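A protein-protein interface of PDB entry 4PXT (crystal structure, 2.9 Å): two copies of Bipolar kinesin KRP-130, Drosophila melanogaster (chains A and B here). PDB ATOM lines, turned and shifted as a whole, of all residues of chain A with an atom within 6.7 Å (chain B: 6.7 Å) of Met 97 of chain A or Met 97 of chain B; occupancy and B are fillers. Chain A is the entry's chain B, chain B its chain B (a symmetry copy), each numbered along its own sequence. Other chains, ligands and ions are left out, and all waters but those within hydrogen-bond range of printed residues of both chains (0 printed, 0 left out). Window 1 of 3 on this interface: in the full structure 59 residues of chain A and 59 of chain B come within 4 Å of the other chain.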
ATOM      1  N   ALA A  92     -22.630  10.188 -10.522  1.00  0.00           N
ATOM      2  CA  ALA A  92     -21.543  11.154 -10.469  1.00  0.00           C
ATOM      3  C   ALA A  92     -21.942  12.371  -9.647  1.00  0.00           C
ATOM      4  O   ALA A  92     -21.131  12.906  -8.890  1.00  0.00           O
ATOM      5  CB  ALA A  92     -21.140  11.568 -11.866  1.00  0.00           C
ATOM      6  N   LEU A  93     -23.194  12.797  -9.797  1.00  0.00           N
ATOM      7  CA  LEU A  93     -23.725  13.952  -9.073  1.00  0.00           C
ATOM      8  C   LEU A  93     -23.714  13.695  -7.569  1.00  0.00           C
ATOM      9  O   LEU A  93     -23.077  14.410  -6.803  1.00  0.00           O
ATOM     10  CB  LEU A  93     -25.151  14.269  -9.532  1.00  0.00           C
ATOM     11  CG  LEU A  93     -25.826  15.518  -8.961  1.00  0.00           C
ATOM     12  CD1 LEU A  93     -25.173  16.759  -9.541  1.00  0.00           C
ATOM     13  CD2 LEU A  93     -27.341  15.516  -9.218  1.00  0.00           C
ATOM     14  N   LEU A  94     -24.450  12.667  -7.176  1.00  0.00           N
ATOM     15  CA  LEU A  94     -24.533  12.199  -5.805  1.00  0.00           C
ATOM     16  C   LEU A  94     -23.187  12.044  -5.111  1.00  0.00           C
ATOM     17  O   LEU A  94     -22.985  12.551  -4.018  1.00  0.00           O
ATOM     18  CB  LEU A  94     -25.269  10.869  -5.791  1.00  0.00           C
ATOM     19  CG  LEU A  94     -26.231  10.659  -4.637  1.00  0.00           C
ATOM     20  CD1 LEU A  94     -26.845  11.982  -4.230  1.00  0.00           C
ATOM     21  CD2 LEU A  94     -27.317   9.678  -5.060  1.00  0.00           C
ATOM     22  N   GLU A  95     -22.266  11.344  -5.756  1.00  0.00           N
ATOM     23  CA  GLU A  95     -20.939  11.144  -5.210  1.00  0.00           C
ATOM     24  C   GLU A  95     -20.224  12.480  -5.097  1.00  0.00           C
ATOM     25  O   GLU A  95     -19.474  12.720  -4.152  1.00  0.00           O
ATOM     26  CB  GLU A  95     -20.143  10.178  -6.092  1.00  0.00           C
ATOM     27  CG  GLU A  95     -18.741   9.856  -5.592  1.00  0.00           C
ATOM     28  CD  GLU A  95     -17.875   9.200  -6.666  1.00  0.00           C
ATOM     29  OE1 GLU A  95     -18.440   8.683  -7.663  1.00  0.00           O
ATOM     30  OE2 GLU A  95     -16.630   9.199  -6.510  1.00  0.00           O
ATOM     31  N   SER A  96     -20.466  13.356  -6.063  1.00  0.00           N
ATOM     32  CA  SER A  96     -19.861  14.674  -6.034  1.00  0.00           C
ATOM     33  C   SER A  96     -20.391  15.465  -4.852  1.00  0.00           C
ATOM     34  O   SER A  96     -19.617  15.972  -4.046  1.00  0.00           O
ATOM     35  CB  SER A  96     -20.120  15.435  -7.329  1.00  0.00           C
ATOM     36  OG  SER A  96     -19.328  16.606  -7.392  1.00  0.00           O
ATOM     37  N   MET A  97     -21.712  15.560  -4.735  1.00  0.00           N
ATOM     38  CA  MET A  97     -22.298  16.435  -3.728  1.00  0.00           C
ATOM     39  C   MET A  97     -22.224  15.797  -2.351  1.00  0.00           C
ATOM     40  O   MET A  97     -22.416  16.469  -1.344  1.00  0.00           O
ATOM     41  CB  MET A  97     -23.748  16.772  -4.075  1.00  0.00           C
ATOM     42  CG  MET A  97     -24.756  15.709  -3.659  1.00  0.00           C
ATOM     43  SD  MET A  97     -25.434  15.925  -1.839  1.00  0.00           S
ATOM     44  CE  MET A  97     -26.570  14.366  -1.739  1.00  0.00           C
ATOM     45  N   MET A  98     -21.934  14.504  -2.300  1.00  0.00           N
ATOM     46  CA  MET A  98     -21.686  13.849  -1.019  1.00  0.00           C
ATOM     47  C   MET A  98     -20.308  14.165  -0.490  1.00  0.00           C
ATOM     48  O   MET A  98     -20.127  14.379   0.703  1.00  0.00           O
ATOM     49  CB  MET A  98     -21.825  12.341  -1.150  1.00  0.00           C
ATOM     50  CG  MET A  98     -23.207  11.827  -0.901  1.00  0.00           C
ATOM     51  SD  MET A  98     -23.631  11.873   0.986  1.00  0.00           S
ATOM     52  CE  MET A  98     -24.713  13.481   0.954  1.00  0.00           C
ATOM     53  N   MET A  99     -19.338  14.196  -1.394  1.00  0.00           N
ATOM     54  CA  MET A  99     -17.962  14.430  -1.009  1.00  0.00           C
ATOM     55  C   MET A  99     -17.838  15.828  -0.435  1.00  0.00           C
ATOM     56  O   MET A  99     -17.164  16.040   0.575  1.00  0.00           O
ATOM     57  CB  MET A  99     -17.030  14.253  -2.203  1.00  0.00           C
ATOM     58  CG  MET A  99     -15.587  14.558  -1.896  1.00  0.00           C
ATOM     59  SD  MET A  99     -14.428  13.918  -3.309  1.00  0.00           S
ATOM     60  CE  MET A  99     -15.140  14.986  -4.782  1.00  0.00           C
ATOM     61  N   GLN A 100     -18.515  16.780  -1.066  1.00  0.00           N
ATOM     62  CA  GLN A 100     -18.477  18.151  -0.591  1.00  0.00           C
ATOM     63  C   GLN A 100     -19.183  18.238   0.763  1.00  0.00           C
ATOM     64  O   GLN A 100     -18.661  18.855   1.692  1.00  0.00           O
ATOM     65  CB  GLN A 100     -19.091  19.097  -1.628  1.00  0.00           C
ATOM     66  CG  GLN A 100     -18.494  18.905  -3.026  1.00  0.00           C
ATOM     67  CD  GLN A 100     -18.574  20.147  -3.902  1.00  0.00           C
ATOM     68  OE1 GLN A 100     -19.425  20.247  -4.789  1.00  0.00           O
ATOM     69  NE2 GLN A 100     -17.665  21.087  -3.674  1.00  0.00           N
ATOM     70  N   MET A 101     -20.355  17.615   0.877  1.00  0.00           N
ATOM     71  CA  MET A 101     -21.050  17.492   2.163  1.00  0.00           C
ATOM     72  C   MET A 101     -20.161  16.962   3.276  1.00  0.00           C
ATOM     73  O   MET A 101     -20.257  17.404   4.423  1.00  0.00           O
ATOM     74  CB  MET A 101     -22.259  16.575   2.045  1.00  0.00           C
ATOM     75  CG  MET A 101     -23.470  17.259   1.506  1.00  0.00           C
ATOM     76  SD  MET A 101     -24.050  18.606   2.739  1.00  0.00           S
ATOM     77  CE  MET A 101     -25.584  19.238   1.709  1.00  0.00           C
ATOM     78  N   GLU A 102     -19.294  16.018   2.925  1.00  0.00           N
ATOM     79  CA  GLU A 102     -18.359  15.433   3.873  1.00  0.00           C
ATOM     80  C   GLU A 102     -17.284  16.444   4.271  1.00  0.00           C
ATOM     81  O   GLU A 102     -17.011  16.623   5.457  1.00  0.00           O
ATOM     82  CB  GLU A 102     -17.730  14.171   3.270  1.00  0.00           C
ATOM     83  CG  GLU A 102     -16.709  13.443   4.148  1.00  0.00           C
ATOM     84  CD  GLU A 102     -17.343  12.743   5.335  1.00  0.00           C
ATOM     85  OE1 GLU A 102     -18.553  12.426   5.261  1.00  0.00           O
ATOM     86  OE2 GLU A 102     -16.626  12.502   6.333  1.00  0.00           O
ATOM     87  N   ALA B  92     -26.147  26.479  -0.393  1.00  0.00           N
ATOM     88  CA  ALA B  92     -25.864  26.656  -1.810  1.00  0.00           C
ATOM     89  C   ALA B  92     -25.616  25.314  -2.483  1.00  0.00           C
ATOM     90  O   ALA B  92     -26.052  25.091  -3.613  1.00  0.00           O
ATOM     91  CB  ALA B  92     -24.676  27.571  -1.998  1.00  0.00           C
ATOM     92  N   LEU B  93     -24.919  24.424  -1.779  1.00  0.00           N
ATOM     93  CA  LEU B  93     -24.602  23.090  -2.291  1.00  0.00           C
ATOM     94  C   LEU B  93     -25.878  22.291  -2.535  1.00  0.00           C
ATOM     95  O   LEU B  93     -26.165  21.868  -3.650  1.00  0.00           O
ATOM     96  CB  LEU B  93     -23.699  22.337  -1.310  1.00  0.00           C
ATOM     97  CG  LEU B  93     -23.173  20.963  -1.733  1.00  0.00           C
ATOM     98  CD1 LEU B  93     -22.141  21.130  -2.832  1.00  0.00           C
ATOM     99  CD2 LEU B  93     -22.596  20.182  -0.542  1.00  0.00           C
ATOM    100  N   LEU B  94     -26.619  22.085  -1.456  1.00  0.00           N
ATOM    101  CA  LEU B  94     -27.904  21.411  -1.465  1.00  0.00           C
ATOM    102  C   LEU B  94     -28.859  21.892  -2.548  1.00  0.00           C
ATOM    103  O   LEU B  94     -29.405  21.097  -3.298  1.00  0.00           O
ATOM    104  CB  LEU B  94     -28.550  21.586  -0.101  1.00  0.00           C
ATOM    105  CG  LEU B  94     -29.289  20.376   0.440  1.00  0.00           C
ATOM    106  CD1 LEU B  94     -28.612  19.105  -0.031  1.00  0.00           C
ATOM    107  CD2 LEU B  94     -29.307  20.435   1.962  1.00  0.00           C
ATOM    108  N   GLU B  95     -29.052  23.200  -2.627  1.00  0.00           N
ATOM    109  CA  GLU B  95     -29.921  23.783  -3.630  1.00  0.00           C
ATOM    110  C   GLU B  95     -29.359  23.513  -5.016  1.00  0.00           C
ATOM    111  O   GLU B  95     -30.102  23.279  -5.968  1.00  0.00           O
ATOM    112  CB  GLU B  95     -30.072  25.288  -3.391  1.00  0.00           C
ATOM    113  CG  GLU B  95     -31.002  26.004  -4.361  1.00  0.00           C
ATOM    114  CD  GLU B  95     -30.836  27.521  -4.315  1.00  0.00           C
ATOM    115  OE1 GLU B  95     -30.273  28.037  -3.315  1.00  0.00           O
ATOM    116  OE2 GLU B  95     -31.271  28.199  -5.278  1.00  0.00           O
ATOM    117  N   SER B  96     -28.037  23.539  -5.125  1.00  0.00           N
ATOM    118  CA  SER B  96     -27.396  23.263  -6.397  1.00  0.00           C
ATOM    119  C   SER B  96     -27.643  21.822  -6.803  1.00  0.00           C
ATOM    120  O   SER B  96     -28.124  21.559  -7.901  1.00  0.00           O
ATOM    121  CB  SER B  96     -25.897  23.537  -6.335  1.00  0.00           C
ATOM    122  OG  SER B  96     -25.326  23.504  -7.630  1.00  0.00           O
ATOM    123  N   MET B  97     -27.333  20.883  -5.913  1.00  0.00           N
ATOM    124  CA  MET B  97     -27.385  19.475  -6.285  1.00  0.00           C
ATOM    125  C   MET B  97     -28.819  18.976  -6.306  1.00  0.00           C
ATOM    126  O   MET B  97     -29.098  17.911  -6.844  1.00  0.00           O
ATOM    127  CB  MET B  97     -26.546  18.628  -5.329  1.00  0.00           C
ATOM    128  CG  MET B  97     -27.256  18.256  -4.033  1.00  0.00           C
ATOM    129  SD  MET B  97     -28.296  16.605  -4.142  1.00  0.00           S
ATOM    130  CE  MET B  97     -29.046  16.588  -2.362  1.00  0.00           C
ATOM    131  N   MET B  98     -29.735  19.747  -5.734  1.00  0.00           N
ATOM    132  CA  MET B  98     -31.154  19.424  -5.849  1.00  0.00           C
ATOM    133  C   MET B  98     -31.703  19.801  -7.204  1.00  0.00           C
ATOM    134  O   MET B  98     -32.500  19.072  -7.783  1.00  0.00           O
ATOM    135  CB  MET B  98     -31.958  20.145  -4.779  1.00  0.00           C
ATOM    136  CG  MET B  98     -32.107  19.380  -3.502  1.00  0.00           C
ATOM    137  SD  MET B  98     -33.367  17.927  -3.712  1.00  0.00           S
ATOM    138  CE  MET B  98     -32.067  16.502  -3.897  1.00  0.00           C
ATOM    139  N   MET B  99     -31.263  20.947  -7.704  1.00  0.00           N
ATOM    140  CA  MET B  99     -31.755  21.451  -8.969  1.00  0.00           C
ATOM    141  C   MET B  99     -31.344  20.500 -10.077  1.00  0.00           C
ATOM    142  O   MET B  99     -32.134  20.192 -10.971  1.00  0.00           O
ATOM    143  CB  MET B  99     -31.220  22.854  -9.237  1.00  0.00           C
ATOM    144  CG  MET B  99     -31.628  23.413 -10.576  1.00  0.00           C
ATOM    145  SD  MET B  99     -31.277  25.314 -10.667  1.00  0.00           S
ATOM    146  CE  MET B  99     -29.340  25.270 -10.415  1.00  0.00           C
ATOM    147  N   GLN B 100     -30.112  20.012  -9.998  1.00  0.00           N
ATOM    148  CA  GLN B 100     -29.622  19.082 -10.999  1.00  0.00           C
ATOM    149  C   GLN B 100     -30.391  17.764 -10.885  1.00  0.00           C
ATOM    150  O   GLN B 100     -30.829  17.216 -11.897  1.00  0.00           O
ATOM    151  CB  GLN B 100     -28.109  18.887 -10.858  1.00  0.00           C
ATOM    152  CG  GLN B 100     -27.346  20.214 -10.814  1.00  0.00           C
ATOM    153  CD  GLN B 100     -25.906  20.109 -11.294  1.00  0.00           C
ATOM    154  OE1 GLN B 100     -24.968  20.082 -10.493  1.00  0.00           O
ATOM    155  NE2 GLN B 100     -25.724  20.080 -12.609  1.00  0.00           N
ATOM    156  N   MET B 101     -30.561  17.265  -9.662  1.00  0.00           N
ATOM    157  CA  MET B 101     -31.411  16.097  -9.408  1.00  0.00           C
ATOM    158  C   MET B 101     -32.793  16.216 -10.031  1.00  0.00           C
ATOM    159  O   MET B 101     -33.343  15.234 -10.534  1.00  0.00           O
ATOM    160  CB  MET B 101     -31.584  15.861  -7.914  1.00  0.00           C
ATOM    161  CG  MET B 101     -30.449  15.113  -7.299  1.00  0.00           C
ATOM    162  SD  MET B 101     -30.377  13.342  -8.026  1.00  0.00           S
ATOM    163  CE  MET B 101     -28.828  12.722  -7.011  1.00  0.00           C
ATOM    164  N   GLU B 102     -33.342  17.426  -9.997  1.00  0.00           N
ATOM    165  CA  GLU B 102     -34.647  17.702 -10.576  1.00  0.00           C
ATOM    166  C   GLU B 102     -34.589  17.636 -12.102  1.00  0.00           C
ATOM    167  O   GLU B 102     -35.427  16.986 -12.725  1.00  0.00           O
ATOM    168  CB  GLU B 102     -35.146  19.073 -10.103  1.00  0.00           C
ATOM    169  CG  GLU B 102     -36.510  19.514 -10.638  1.00  0.00           C
ATOM    170  CD  GLU B 102     -37.661  18.723 -10.047  1.00  0.00           C
ATOM    171  OE1 GLU B 102     -37.493  18.170  -8.936  1.00  0.00           O
ATOM    172  OE2 GLU B 102     -38.734  18.667 -10.691  1.00  0.00           O
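The side-chain sulfur of Met 97 of chain A lies close to the side-chain sulfur of Met 97 of chain B.
Among the printed residues, merely in contact across the chains: Gln 100 of chain A with Leu 93 of chain B (3.5 Å), Leu 93 of chain A with Gln 100 of chain B (3.5 Å), Leu 94 of chain A with Met 101 of chain B (3.5 Å), Met 101 of chain A with Leu 94 of chain B (3.5 Å), Met 101 of chain A with Leu 93 of chain B (3.7 Å), Leu 93 of chain A with Met 101 of chain B (3.7 Å), Leu 93 of chain A with Met 97 of chain B (3.8 Å) and Met 97 of chain A with Leu 93 of chain B (3.8 Å).
Ala 92 of chain A touches none of the printed residues of chain B. Of the printed residues of chain B, Leu 94 of chain A touches Met 101. Of the printed residues of chain B, Met 97 of chain A touches Leu 93 and Met 97. Met 99 of chain A touches none of the printed residues of chain B. Printed residues of chain B within 4 Å of Met 101 of chain A: Leu 93 and Leu 94. Printed residues of chain A within 4 Å of Leu 93 of chain B: Met 97, Gln 100 and Met 101. Of chain A, only Leu 93 (3.8 Å) and Met 97 (3.4 Å) come within 4 Å of Met 97 of chain B.
Of the 11 printed residues of chain A, 5 touch a printed residue of chain B. Printed residues of chain A that touch a printed residue of chain B: Leu 93, Leu 94, Met 97, Gln 100 and Met 101. Hydrophobic or aromatic side chains of chain A within 4 Å of the printed part of chain B: Leu 93, Leu 94, Met 97 and Met 101. Of the 11 printed residues of chain B, 5 touch a printed residue of chain A. Hydrophobic or aromatic side chains of chain B that line the printed part of chain A: Leu 93, Leu 94, Met 97 and Met 101. Among the printed residues, no Asp or Glu carboxylate lies within 4 Å of a Lys or Arg side-chain nitrogen of the other chain.
Leu 93 of chain A touches Gln 100 of chain B, and with the chains exchanged Gln 100 of chain A touches Leu 93 of chain B. Leu 93 of chain A touches Met 101 of chain B, and with the chains exchanged Met 101 of chain A touches Leu 93 of chain B. Leu 94 of chain A touches Met 101 of chain B, and with the chains exchanged Met 101 of chain A touches Leu 94 of chain B. Met 97 of chain A touches its own counterpart, Met 97 of chain B. 11 positions are printed for both chains.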
